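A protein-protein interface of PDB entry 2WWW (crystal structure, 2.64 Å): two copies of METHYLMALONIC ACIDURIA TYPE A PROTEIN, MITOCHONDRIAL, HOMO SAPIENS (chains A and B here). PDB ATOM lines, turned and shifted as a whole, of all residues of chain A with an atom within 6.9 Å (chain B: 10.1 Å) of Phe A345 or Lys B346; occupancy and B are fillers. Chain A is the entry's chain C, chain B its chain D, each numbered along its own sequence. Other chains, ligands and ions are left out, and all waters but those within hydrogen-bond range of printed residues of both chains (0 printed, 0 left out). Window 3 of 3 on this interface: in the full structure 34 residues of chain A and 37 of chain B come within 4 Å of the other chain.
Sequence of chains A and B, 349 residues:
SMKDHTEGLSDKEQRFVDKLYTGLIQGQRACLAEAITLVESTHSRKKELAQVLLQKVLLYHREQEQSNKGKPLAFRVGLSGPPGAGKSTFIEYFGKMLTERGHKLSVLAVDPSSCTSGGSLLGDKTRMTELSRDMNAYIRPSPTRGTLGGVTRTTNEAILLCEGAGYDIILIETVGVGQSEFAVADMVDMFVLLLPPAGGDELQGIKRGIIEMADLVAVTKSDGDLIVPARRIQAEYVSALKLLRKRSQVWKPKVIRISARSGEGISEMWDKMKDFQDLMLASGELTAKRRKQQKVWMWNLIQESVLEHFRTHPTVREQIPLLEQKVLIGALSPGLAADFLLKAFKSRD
The side-chain carboxylate (OD1) of Asp B339 is in hydrogen-bond range of a ring nitrogen (ND1) of His A309, 2.9 Å away.
Val A306 touches Ala B338 (N to CB, 3.6 Å).
CG1 of Val A306 touches CD2 of Leu B342, 3.9 Å away.
Leu B342 touches His A309 (CD1 to CB, 3.5 Å).
CE2 of Phe A310 touches CG1 of Val B306, 3.7 Å away.
Arg A311 touches Trp B299.
Leu A342 touches Val B306.
CD2 of Leu A342 touches CZ of Phe B345, 3.8 Å away.
Leu B342 touches Phe A345 (CD2 to CZ, 3.98 Å).
Phe A345 touches Lys B346 (CE2 to CD, 3.6 Å).
Phe B345 touches Lys A346 (CE2 to CE, 3.6 Å).
Of the printed residues of chain B, Val A306 touches Phe B310, Ala B338 and Leu B342.
Of chain B, only Val B306 comes within 4 Å of Phe A310.
Printed residues of chain B within 4 Å of Arg A311: Trp B299 (3.9 Å).
No residue of chain B comes within 4 Å of Ala A344.
Of the printed residues of chain B, Phe A345 touches Leu B342 (3.98 Å) and Lys B346 (3.6 Å).
Of chain B, only Phe B345 (3.6 Å) comes within 4 Å of Lys A346.
No residue of chain B comes within 4 Å of Ser A347.
Of the printed residues of chain A, Phe B310 touches Val A306.
Val B316 touches none of the printed residues of chain A.
Of the printed residues of chain A, Asp B339 touches His A309.
Ser B347 touches none of the printed residues of chain A.
The nearest printed residue of chain B that does not touch Phe A345 is Phe B345 (5.0 Å).
The nearest residue of chain A that does not touch Lys B346 is Lys A346 (4.05 Å).
Of the 15 printed residues of chain A, 7 touch a printed residue of chain B.
Along chain A the printed residues that touch a printed residue of chain B span positions 306 to 346.
Of the 17 printed residues of chain B, 8 touch a printed residue of chain A.
Val A306 touches Phe B310, and with the chains exchanged Phe A310 touches Val B306.
Val A306 touches Leu B342, and with the chains exchanged Leu A342 touches Val B306.
Leu A342 touches Phe B345, and with the chains exchanged Phe A345 touches Leu B342.
Phe A345 touches Lys B346, and with the chains exchanged Lys A346 touches Phe B345.
13 positions are printed for both chains.
Of the 12 pairs that touch across the chains among the printed residues, 8 have their exchanged pair printed and touching as well.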
ATOM      1  N   VAL A 306     -14.642 -20.290  -8.967  1.00  0.00           N
ATOM      2  CA  VAL A 306     -13.637 -20.670  -9.972  1.00  0.00           C
ATOM      3  C   VAL A 306     -13.520 -22.189  -9.980  1.00  0.00           C
ATOM      4  O   VAL A 306     -13.632 -22.789 -11.044  1.00  0.00           O
ATOM      5  CB  VAL A 306     -12.251 -19.937  -9.805  1.00  0.00           C
ATOM      6  CG1 VAL A 306     -11.193 -20.526 -10.727  1.00  0.00           C
ATOM      7  CG2 VAL A 306     -12.366 -18.405 -10.017  1.00  0.00           C
ATOM      8  N   HIS A 309     -16.830 -24.241 -11.270  1.00  0.00           N
ATOM      9  CA  HIS A 309     -16.881 -24.096 -12.724  1.00  0.00           C
ATOM     10  C   HIS A 309     -15.822 -24.964 -13.392  1.00  0.00           C
ATOM     11  O   HIS A 309     -16.134 -25.684 -14.331  1.00  0.00           O
ATOM     12  CB  HIS A 309     -16.759 -22.620 -13.154  1.00  0.00           C
ATOM     13  CG  HIS A 309     -17.829 -21.674 -12.640  1.00  0.00           C
ATOM     14  ND1 HIS A 309     -17.906 -20.368 -13.096  1.00  0.00           N
ATOM     15  CD2 HIS A 309     -18.796 -21.860 -11.699  1.00  0.00           C
ATOM     16  CE1 HIS A 309     -18.914 -19.810 -12.435  1.00  0.00           C
ATOM     17  NE2 HIS A 309     -19.487 -20.671 -11.592  1.00  0.00           N
ATOM     18  N   PHE A 310     -14.612 -24.977 -12.872  1.00  0.00           N
ATOM     19  CA  PHE A 310     -13.495 -25.772 -13.348  1.00  0.00           C
ATOM     20  C   PHE A 310     -13.712 -27.294 -13.191  1.00  0.00           C
ATOM     21  O   PHE A 310     -13.526 -28.040 -14.164  1.00  0.00           O
ATOM     22  CB  PHE A 310     -12.225 -25.351 -12.598  1.00  0.00           C
ATOM     23  CG  PHE A 310     -10.967 -25.969 -13.147  1.00  0.00           C
ATOM     24  CD1 PHE A 310     -10.395 -25.497 -14.335  1.00  0.00           C
ATOM     25  CD2 PHE A 310     -10.347 -27.038 -12.491  1.00  0.00           C
ATOM     26  CE1 PHE A 310      -9.217 -26.079 -14.851  1.00  0.00           C
ATOM     27  CE2 PHE A 310      -9.174 -27.621 -13.012  1.00  0.00           C
ATOM     28  CZ  PHE A 310      -8.612 -27.129 -14.179  1.00  0.00           C
ATOM     29  N   ARG A 311     -14.046 -27.771 -11.957  1.00  0.00           N
ATOM     30  CA  ARG A 311     -14.218 -29.209 -11.641  1.00  0.00           C
ATOM     31  C   ARG A 311     -15.462 -29.843 -12.309  1.00  0.00           C
ATOM     32  O   ARG A 311     -15.584 -31.090 -12.345  1.00  0.00           O
ATOM     33  CB  ARG A 311     -14.158 -29.468 -10.119  1.00  0.00           C
ATOM     34  CG  ARG A 311     -15.497 -29.330  -9.425  1.00  0.00           C
ATOM     35  CD  ARG A 311     -15.492 -29.800  -7.985  1.00  0.00           C
ATOM     36  NE  ARG A 311     -15.943 -28.735  -7.081  1.00  0.00           N
ATOM     37  CZ  ARG A 311     -15.149 -28.066  -6.245  1.00  0.00           C
ATOM     38  NH1 ARG A 311     -13.855 -28.368  -6.153  1.00  0.00           N
ATOM     39  NH2 ARG A 311     -15.645 -27.105  -5.476  1.00  0.00           N
ATOM     40  N   HIS A 313     -16.493 -28.805 -15.623  1.00  0.00           N
ATOM     41  CA  HIS A 313     -16.227 -28.702 -17.062  1.00  0.00           C
ATOM     42  C   HIS A 313     -15.919 -30.107 -17.599  1.00  0.00           C
ATOM     43  O   HIS A 313     -15.095 -30.809 -16.997  1.00  0.00           O
ATOM     44  CB  HIS A 313     -15.044 -27.746 -17.241  1.00  0.00           C
ATOM     45  CG  HIS A 313     -14.584 -27.510 -18.634  1.00  0.00           C
ATOM     46  ND1 HIS A 313     -13.694 -28.382 -19.259  1.00  0.00           N
ATOM     47  CD2 HIS A 313     -14.777 -26.430 -19.430  1.00  0.00           C
ATOM     48  CE1 HIS A 313     -13.412 -27.833 -20.433  1.00  0.00           C
ATOM     49  NE2 HIS A 313     -14.018 -26.643 -20.573  1.00  0.00           N
ATOM     50  N   THR A 315     -14.086 -31.617 -19.811  1.00  0.00           N
ATOM     51  CA  THR A 315     -12.734 -32.137 -20.088  1.00  0.00           C
ATOM     52  C   THR A 315     -11.998 -32.463 -18.803  1.00  0.00           C
ATOM     53  O   THR A 315     -11.518 -33.593 -18.614  1.00  0.00           O
ATOM     54  CB  THR A 315     -11.991 -31.389 -21.227  1.00  0.00           C
ATOM     55  OG1 THR A 315     -12.794 -31.455 -22.421  1.00  0.00           O
ATOM     56  CG2 THR A 315     -10.606 -32.012 -21.529  1.00  0.00           C
ATOM     57  N   VAL A 316     -12.057 -31.520 -17.876  1.00  0.00           N
ATOM     58  CA  VAL A 316     -11.563 -31.633 -16.495  1.00  0.00           C
ATOM     59  C   VAL A 316     -12.226 -32.877 -15.807  1.00  0.00           C
ATOM     60  O   VAL A 316     -11.529 -33.829 -15.514  1.00  0.00           O
ATOM     61  CB  VAL A 316     -11.774 -30.286 -15.756  1.00  0.00           C
ATOM     62  CG1 VAL A 316     -11.230 -30.344 -14.345  1.00  0.00           C
ATOM     63  CG2 VAL A 316     -11.136 -29.125 -16.534  1.00  0.00           C
ATOM     64  N   PHE A 340      -1.490 -29.574 -17.100  1.00  0.00           N
ATOM     65  CA  PHE A 340      -2.228 -30.348 -18.079  1.00  0.00           C
ATOM     66  C   PHE A 340      -3.704 -29.940 -18.058  1.00  0.00           C
ATOM     67  O   PHE A 340      -4.176 -29.456 -19.085  1.00  0.00           O
ATOM     68  CB  PHE A 340      -2.015 -31.858 -17.871  1.00  0.00           C
ATOM     69  CG  PHE A 340      -2.930 -32.709 -18.713  1.00  0.00           C
ATOM     70  CD1 PHE A 340      -2.696 -32.880 -20.064  1.00  0.00           C
ATOM     71  CD2 PHE A 340      -4.041 -33.323 -18.152  1.00  0.00           C
ATOM     72  CE1 PHE A 340      -3.574 -33.645 -20.843  1.00  0.00           C
ATOM     73  CE2 PHE A 340      -4.893 -34.111 -18.916  1.00  0.00           C
ATOM     74  CZ  PHE A 340      -4.658 -34.271 -20.255  1.00  0.00           C
ATOM     75  N   LEU A 341      -4.399 -30.053 -16.898  1.00  0.00           N
ATOM     76  CA  LEU A 341      -5.800 -29.681 -16.722  1.00  0.00           C
ATOM     77  C   LEU A 341      -6.139 -28.247 -17.134  1.00  0.00           C
ATOM     78  O   LEU A 341      -7.141 -28.030 -17.830  1.00  0.00           O
ATOM     79  CB  LEU A 341      -6.243 -29.904 -15.281  1.00  0.00           C
ATOM     80  CG  LEU A 341      -6.611 -31.340 -14.923  1.00  0.00           C
ATOM     81  CD1 LEU A 341      -7.079 -31.402 -13.495  1.00  0.00           C
ATOM     82  CD2 LEU A 341      -7.634 -31.974 -15.919  1.00  0.00           C
ATOM     83  N   LEU A 342      -5.316 -27.279 -16.713  1.00  0.00           N
ATOM     84  CA  LEU A 342      -5.497 -25.900 -17.095  1.00  0.00           C
ATOM     85  C   LEU A 342      -5.425 -25.740 -18.632  1.00  0.00           C
ATOM     86  O   LEU A 342      -6.310 -25.089 -19.198  1.00  0.00           O
ATOM     87  CB  LEU A 342      -4.526 -24.975 -16.352  1.00  0.00           C
ATOM     88  CG  LEU A 342      -4.802 -24.782 -14.838  1.00  0.00           C
ATOM     89  CD1 LEU A 342      -3.606 -24.249 -14.117  1.00  0.00           C
ATOM     90  CD2 LEU A 342      -5.950 -23.833 -14.599  1.00  0.00           C
ATOM     91  N   LYS A 343      -4.456 -26.402 -19.315  1.00  0.00           N
ATOM     92  CA  LYS A 343      -4.324 -26.370 -20.777  1.00  0.00           C
ATOM     93  C   LYS A 343      -5.542 -27.014 -21.438  1.00  0.00           C
ATOM     94  O   LYS A 343      -6.102 -26.417 -22.358  1.00  0.00           O
ATOM     95  CB  LYS A 343      -3.034 -27.061 -21.229  1.00  0.00           C
ATOM     96  CG  LYS A 343      -1.776 -26.241 -20.956  1.00  0.00           C
ATOM     97  CD  LYS A 343      -0.495 -27.074 -21.017  1.00  0.00           C
ATOM     98  N   ALA A 344      -5.980 -28.205 -20.933  1.00  0.00           N
ATOM     99  CA  ALA A 344      -7.179 -28.935 -21.373  1.00  0.00           C
ATOM    100  C   ALA A 344      -8.448 -28.057 -21.304  1.00  0.00           C
ATOM    101  O   ALA A 344      -9.223 -28.037 -22.244  1.00  0.00           O
ATOM    102  CB  ALA A 344      -7.369 -30.166 -20.522  1.00  0.00           C
ATOM    103  N   PHE A 345      -8.640 -27.318 -20.196  1.00  0.00           N
ATOM    104  CA  PHE A 345      -9.744 -26.380 -19.988  1.00  0.00           C
ATOM    105  C   PHE A 345      -9.700 -25.262 -21.069  1.00  0.00           C
ATOM    106  O   PHE A 345     -10.718 -25.020 -21.726  1.00  0.00           O
ATOM    107  CB  PHE A 345      -9.678 -25.797 -18.562  1.00  0.00           C
ATOM    108  CG  PHE A 345     -10.744 -24.781 -18.254  1.00  0.00           C
ATOM    109  CD1 PHE A 345     -11.965 -25.173 -17.722  1.00  0.00           C
ATOM    110  CD2 PHE A 345     -10.530 -23.430 -18.493  1.00  0.00           C
ATOM    111  CE1 PHE A 345     -12.961 -24.232 -17.452  1.00  0.00           C
ATOM    112  CE2 PHE A 345     -11.524 -22.491 -18.218  1.00  0.00           C
ATOM    113  CZ  PHE A 345     -12.732 -22.900 -17.699  1.00  0.00           C
ATOM    114  N   LYS A 346      -8.518 -24.612 -21.257  1.00  0.00           N
ATOM    115  CA  LYS A 346      -8.256 -23.562 -22.257  1.00  0.00           C
ATOM    116  C   LYS A 346      -8.526 -24.062 -23.726  1.00  0.00           C
ATOM    117  O   LYS A 346      -9.170 -23.348 -24.510  1.00  0.00           O
ATOM    118  CB  LYS A 346      -6.803 -23.055 -22.130  1.00  0.00           C
ATOM    119  CG  LYS A 346      -6.574 -21.990 -21.066  1.00  0.00           C
ATOM    120  CD  LYS A 346      -5.517 -20.955 -21.507  1.00  0.00           C
ATOM    121  CE  LYS A 346      -4.241 -20.926 -20.693  1.00  0.00           C
ATOM    122  NZ  LYS A 346      -3.429 -19.704 -20.983  1.00  0.00           N
ATOM    123  N   SER A 347      -8.022 -25.278 -24.079  1.00  0.00           N
ATOM    124  CA  SER A 347      -8.185 -25.906 -25.396  1.00  0.00           C
ATOM    125  C   SER A 347      -9.387 -26.860 -25.421  1.00  0.00           C
ATOM    126  O   SER A 347     -10.515 -26.466 -25.114  1.00  0.00           O
ATOM    127  CB  SER A 347      -6.921 -26.668 -25.781  1.00  0.00           C
ATOM    128  N   TRP B 299      -6.995 -35.286  -5.517  1.00  0.00           N
ATOM    129  CA  TRP B 299      -7.757 -34.145  -5.959  1.00  0.00           C
ATOM    130  C   TRP B 299      -7.394 -32.855  -5.198  1.00  0.00           C
ATOM    131  O   TRP B 299      -7.260 -31.802  -5.815  1.00  0.00           O
ATOM    132  CB  TRP B 299      -9.277 -34.418  -5.928  1.00  0.00           C
ATOM    133  CG  TRP B 299     -10.071 -33.159  -6.212  1.00  0.00           C
ATOM    134  CD1 TRP B 299     -10.797 -32.441  -5.299  1.00  0.00           C
ATOM    135  CD2 TRP B 299      -9.938 -32.307  -7.376  1.00  0.00           C
ATOM    136  NE1 TRP B 299     -11.217 -31.256  -5.850  1.00  0.00           N
ATOM    137  CE2 TRP B 299     -10.676 -31.129  -7.115  1.00  0.00           C
ATOM    138  CE3 TRP B 299      -9.206 -32.399  -8.586  1.00  0.00           C
ATOM    139  CZ2 TRP B 299     -10.759 -30.074  -8.048  1.00  0.00           C
ATOM    140  CZ3 TRP B 299      -9.284 -31.365  -9.503  1.00  0.00           C
ATOM    141  CH2 TRP B 299     -10.050 -30.219  -9.235  1.00  0.00           C
ATOM    142  N   VAL B 306      -3.767 -26.160  -9.189  1.00  0.00           N
ATOM    143  CA  VAL B 306      -4.666 -25.463 -10.124  1.00  0.00           C
ATOM    144  C   VAL B 306      -4.889 -23.998  -9.638  1.00  0.00           C
ATOM    145  O   VAL B 306      -4.712 -23.081 -10.428  1.00  0.00           O
ATOM    146  CB  VAL B 306      -5.996 -26.221 -10.423  1.00  0.00           C
ATOM    147  CG1 VAL B 306      -6.993 -25.319 -11.165  1.00  0.00           C
ATOM    148  CG2 VAL B 306      -5.735 -27.511 -11.213  1.00  0.00           C
ATOM    149  N   PHE B 310      -3.513 -20.579 -11.307  1.00  0.00           N
ATOM    150  CA  PHE B 310      -4.540 -19.654 -11.723  1.00  0.00           C
ATOM    151  C   PHE B 310      -4.376 -18.259 -11.085  1.00  0.00           C
ATOM    152  O   PHE B 310      -4.278 -17.278 -11.811  1.00  0.00           O
ATOM    153  CB  PHE B 310      -5.931 -20.253 -11.489  1.00  0.00           C
ATOM    154  CG  PHE B 310      -7.077 -19.427 -12.026  1.00  0.00           C
ATOM    155  CD1 PHE B 310      -7.529 -19.598 -13.332  1.00  0.00           C
ATOM    156  CD2 PHE B 310      -7.746 -18.514 -11.206  1.00  0.00           C
ATOM    157  CE1 PHE B 310      -8.616 -18.863 -13.815  1.00  0.00           C
ATOM    158  CE2 PHE B 310      -8.814 -17.760 -11.699  1.00  0.00           C
ATOM    159  CZ  PHE B 310      -9.240 -17.939 -13.001  1.00  0.00           C
ATOM    160  N   HIS B 313      -1.541 -16.198 -12.524  1.00  0.00           N
ATOM    161  CA  HIS B 313      -1.636 -15.872 -13.950  1.00  0.00           C
ATOM    162  C   HIS B 313      -1.782 -14.322 -14.132  1.00  0.00           C
ATOM    163  O   HIS B 313      -2.632 -13.714 -13.494  1.00  0.00           O
ATOM    164  CB  HIS B 313      -2.744 -16.707 -14.632  1.00  0.00           C
ATOM    165  CG  HIS B 313      -2.782 -16.552 -16.107  1.00  0.00           C
ATOM    166  ND1 HIS B 313      -1.756 -16.995 -16.915  1.00  0.00           N
ATOM    167  CD2 HIS B 313      -3.722 -15.959 -16.872  1.00  0.00           C
ATOM    168  CE1 HIS B 313      -2.083 -16.614 -18.143  1.00  0.00           C
ATOM    169  NE2 HIS B 313      -3.261 -15.996 -18.167  1.00  0.00           N
ATOM    170  N   PRO B 314      -0.876 -13.658 -14.870  1.00  0.00           N
ATOM    171  CA  PRO B 314      -0.934 -12.187 -15.006  1.00  0.00           C
ATOM    172  C   PRO B 314      -2.267 -11.521 -15.380  1.00  0.00           C
ATOM    173  O   PRO B 314      -2.573 -10.462 -14.822  1.00  0.00           O
ATOM    174  CB  PRO B 314       0.120 -11.911 -16.077  1.00  0.00           C
ATOM    175  CG  PRO B 314       0.311 -13.217 -16.804  1.00  0.00           C
ATOM    176  CD  PRO B 314       0.226 -14.203 -15.677  1.00  0.00           C
ATOM    177  N   THR B 315      -3.041 -12.107 -16.334  1.00  0.00           N
ATOM    178  CA  THR B 315      -4.363 -11.577 -16.729  1.00  0.00           C
ATOM    179  C   THR B 315      -5.343 -11.720 -15.555  1.00  0.00           C
ATOM    180  O   THR B 315      -6.147 -10.816 -15.331  1.00  0.00           O
ATOM    181  CB  THR B 315      -4.894 -12.194 -18.038  1.00  0.00           C
ATOM    182  OG1 THR B 315      -4.759 -13.607 -17.979  1.00  0.00           O
ATOM    183  CG2 THR B 315      -4.168 -11.711 -19.245  1.00  0.00           C
ATOM    184  N   VAL B 316      -5.187 -12.810 -14.749  1.00  0.00           N
ATOM    185  CA  VAL B 316      -5.969 -13.091 -13.537  1.00  0.00           C
ATOM    186  C   VAL B 316      -5.575 -12.091 -12.424  1.00  0.00           C
ATOM    187  O   VAL B 316      -6.460 -11.384 -11.948  1.00  0.00           O
ATOM    188  CB  VAL B 316      -5.874 -14.574 -13.087  1.00  0.00           C
ATOM    189  CG1 VAL B 316      -6.565 -14.799 -11.747  1.00  0.00           C
ATOM    190  CG2 VAL B 316      -6.455 -15.493 -14.149  1.00  0.00           C
ATOM    191  N   ALA B 338     -16.244 -14.959 -11.013  1.00  0.00           N
ATOM    192  CA  ALA B 338     -15.489 -16.151 -11.401  1.00  0.00           C
ATOM    193  C   ALA B 338     -15.520 -16.383 -12.898  1.00  0.00           C
ATOM    194  O   ALA B 338     -14.465 -16.682 -13.452  1.00  0.00           O
ATOM    195  CB  ALA B 338     -15.981 -17.376 -10.679  1.00  0.00           C
ATOM    196  N   ASP B 339     -16.700 -16.211 -13.557  1.00  0.00           N
ATOM    197  CA  ASP B 339     -16.855 -16.340 -15.014  1.00  0.00           C
ATOM    198  C   ASP B 339     -15.958 -15.340 -15.747  1.00  0.00           C
ATOM    199  O   ASP B 339     -15.232 -15.754 -16.643  1.00  0.00           O
ATOM    200  CB  ASP B 339     -18.325 -16.194 -15.461  1.00  0.00           C
ATOM    201  CG  ASP B 339     -19.151 -17.450 -15.293  1.00  0.00           C
ATOM    202  OD1 ASP B 339     -18.546 -18.550 -15.197  1.00  0.00           O
ATOM    203  OD2 ASP B 339     -20.415 -17.342 -15.302  1.00  0.00           O
ATOM    204  N   PHE B 340     -15.982 -14.035 -15.365  1.00  0.00           N
ATOM    205  CA  PHE B 340     -15.109 -13.015 -15.955  1.00  0.00           C
ATOM    206  C   PHE B 340     -13.618 -13.362 -15.757  1.00  0.00           C
ATOM    207  O   PHE B 340     -12.834 -13.119 -16.666  1.00  0.00           O
ATOM    208  CB  PHE B 340     -15.422 -11.604 -15.419  1.00  0.00           C
ATOM    209  N   LEU B 341     -13.247 -13.985 -14.596  1.00  0.00           N
ATOM    210  CA  LEU B 341     -11.870 -14.409 -14.287  1.00  0.00           C
ATOM    211  C   LEU B 341     -11.392 -15.580 -15.134  1.00  0.00           C
ATOM    212  O   LEU B 341     -10.270 -15.533 -15.674  1.00  0.00           O
ATOM    213  CB  LEU B 341     -11.659 -14.679 -12.797  1.00  0.00           C
ATOM    214  CG  LEU B 341     -11.363 -13.430 -11.932  1.00  0.00           C
ATOM    215  CD1 LEU B 341     -11.109 -13.814 -10.485  1.00  0.00           C
ATOM    216  CD2 LEU B 341     -10.165 -12.635 -12.449  1.00  0.00           C
ATOM    217  N   LEU B 342     -12.260 -16.610 -15.283  1.00  0.00           N
ATOM    218  CA  LEU B 342     -12.023 -17.784 -16.133  1.00  0.00           C
ATOM    219  C   LEU B 342     -11.881 -17.371 -17.618  1.00  0.00           C
ATOM    220  O   LEU B 342     -10.950 -17.843 -18.275  1.00  0.00           O
ATOM    221  CB  LEU B 342     -13.087 -18.871 -15.933  1.00  0.00           C
ATOM    222  CG  LEU B 342     -13.001 -19.628 -14.586  1.00  0.00           C
ATOM    223  CD1 LEU B 342     -14.286 -20.337 -14.270  1.00  0.00           C
ATOM    224  CD2 LEU B 342     -11.848 -20.636 -14.547  1.00  0.00           C
ATOM    225  N   LYS B 343     -12.720 -16.421 -18.112  1.00  0.00           N
ATOM    226  CA  LYS B 343     -12.633 -15.906 -19.483  1.00  0.00           C
ATOM    227  C   LYS B 343     -11.301 -15.212 -19.702  1.00  0.00           C
ATOM    228  O   LYS B 343     -10.641 -15.481 -20.700  1.00  0.00           O
ATOM    229  CB  LYS B 343     -13.802 -14.945 -19.811  1.00  0.00           C
ATOM    230  N   ALA B 344     -10.900 -14.339 -18.753  1.00  0.00           N
ATOM    231  CA  ALA B 344      -9.639 -13.597 -18.749  1.00  0.00           C
ATOM    232  C   ALA B 344      -8.430 -14.551 -18.863  1.00  0.00           C
ATOM    233  O   ALA B 344      -7.532 -14.308 -19.675  1.00  0.00           O
ATOM    234  CB  ALA B 344      -9.543 -12.753 -17.488  1.00  0.00           C
ATOM    235  N   PHE B 345      -8.436 -15.650 -18.074  1.00  0.00           N
ATOM    236  CA  PHE B 345      -7.400 -16.685 -18.090  1.00  0.00           C
ATOM    237  C   PHE B 345      -7.325 -17.345 -19.511  1.00  0.00           C
ATOM    238  O   PHE B 345      -6.235 -17.436 -20.096  1.00  0.00           O
ATOM    239  CB  PHE B 345      -7.685 -17.720 -16.998  1.00  0.00           C
ATOM    240  CG  PHE B 345      -6.712 -18.868 -16.964  1.00  0.00           C
ATOM    241  CD1 PHE B 345      -5.544 -18.791 -16.212  1.00  0.00           C
ATOM    242  CD2 PHE B 345      -6.966 -20.039 -17.665  1.00  0.00           C
ATOM    243  CE1 PHE B 345      -4.647 -19.865 -16.167  1.00  0.00           C
ATOM    244  CE2 PHE B 345      -6.065 -21.103 -17.627  1.00  0.00           C
ATOM    245  CZ  PHE B 345      -4.909 -21.007 -16.890  1.00  0.00           C
ATOM    246  N   LYS B 346      -8.490 -17.769 -20.051  1.00  0.00           N
ATOM    247  CA  LYS B 346      -8.645 -18.393 -21.369  1.00  0.00           C
ATOM    248  C   LYS B 346      -8.151 -17.458 -22.523  1.00  0.00           C
ATOM    249  O   LYS B 346      -7.442 -17.921 -23.424  1.00  0.00           O
ATOM    250  CB  LYS B 346     -10.127 -18.801 -21.590  1.00  0.00           C
ATOM    251  CG  LYS B 346     -10.498 -20.160 -21.008  1.00  0.00           C
ATOM    252  CD  LYS B 346     -11.920 -20.573 -21.297  1.00  0.00           C
ATOM    253  N   SER B 347      -8.532 -16.151 -22.475  1.00  0.00           N
ATOM    254  CA  SER B 347      -8.194 -15.124 -23.461  1.00  0.00           C
ATOM    255  C   SER B 347      -7.001 -14.302 -22.995  1.00  0.00           C
ATOM    256  O   SER B 347      -5.948 -14.862 -22.708  1.00  0.00           O
ATOM    257  CB  SER B 347      -9.395 -14.215 -23.716  1.00  0.00           C
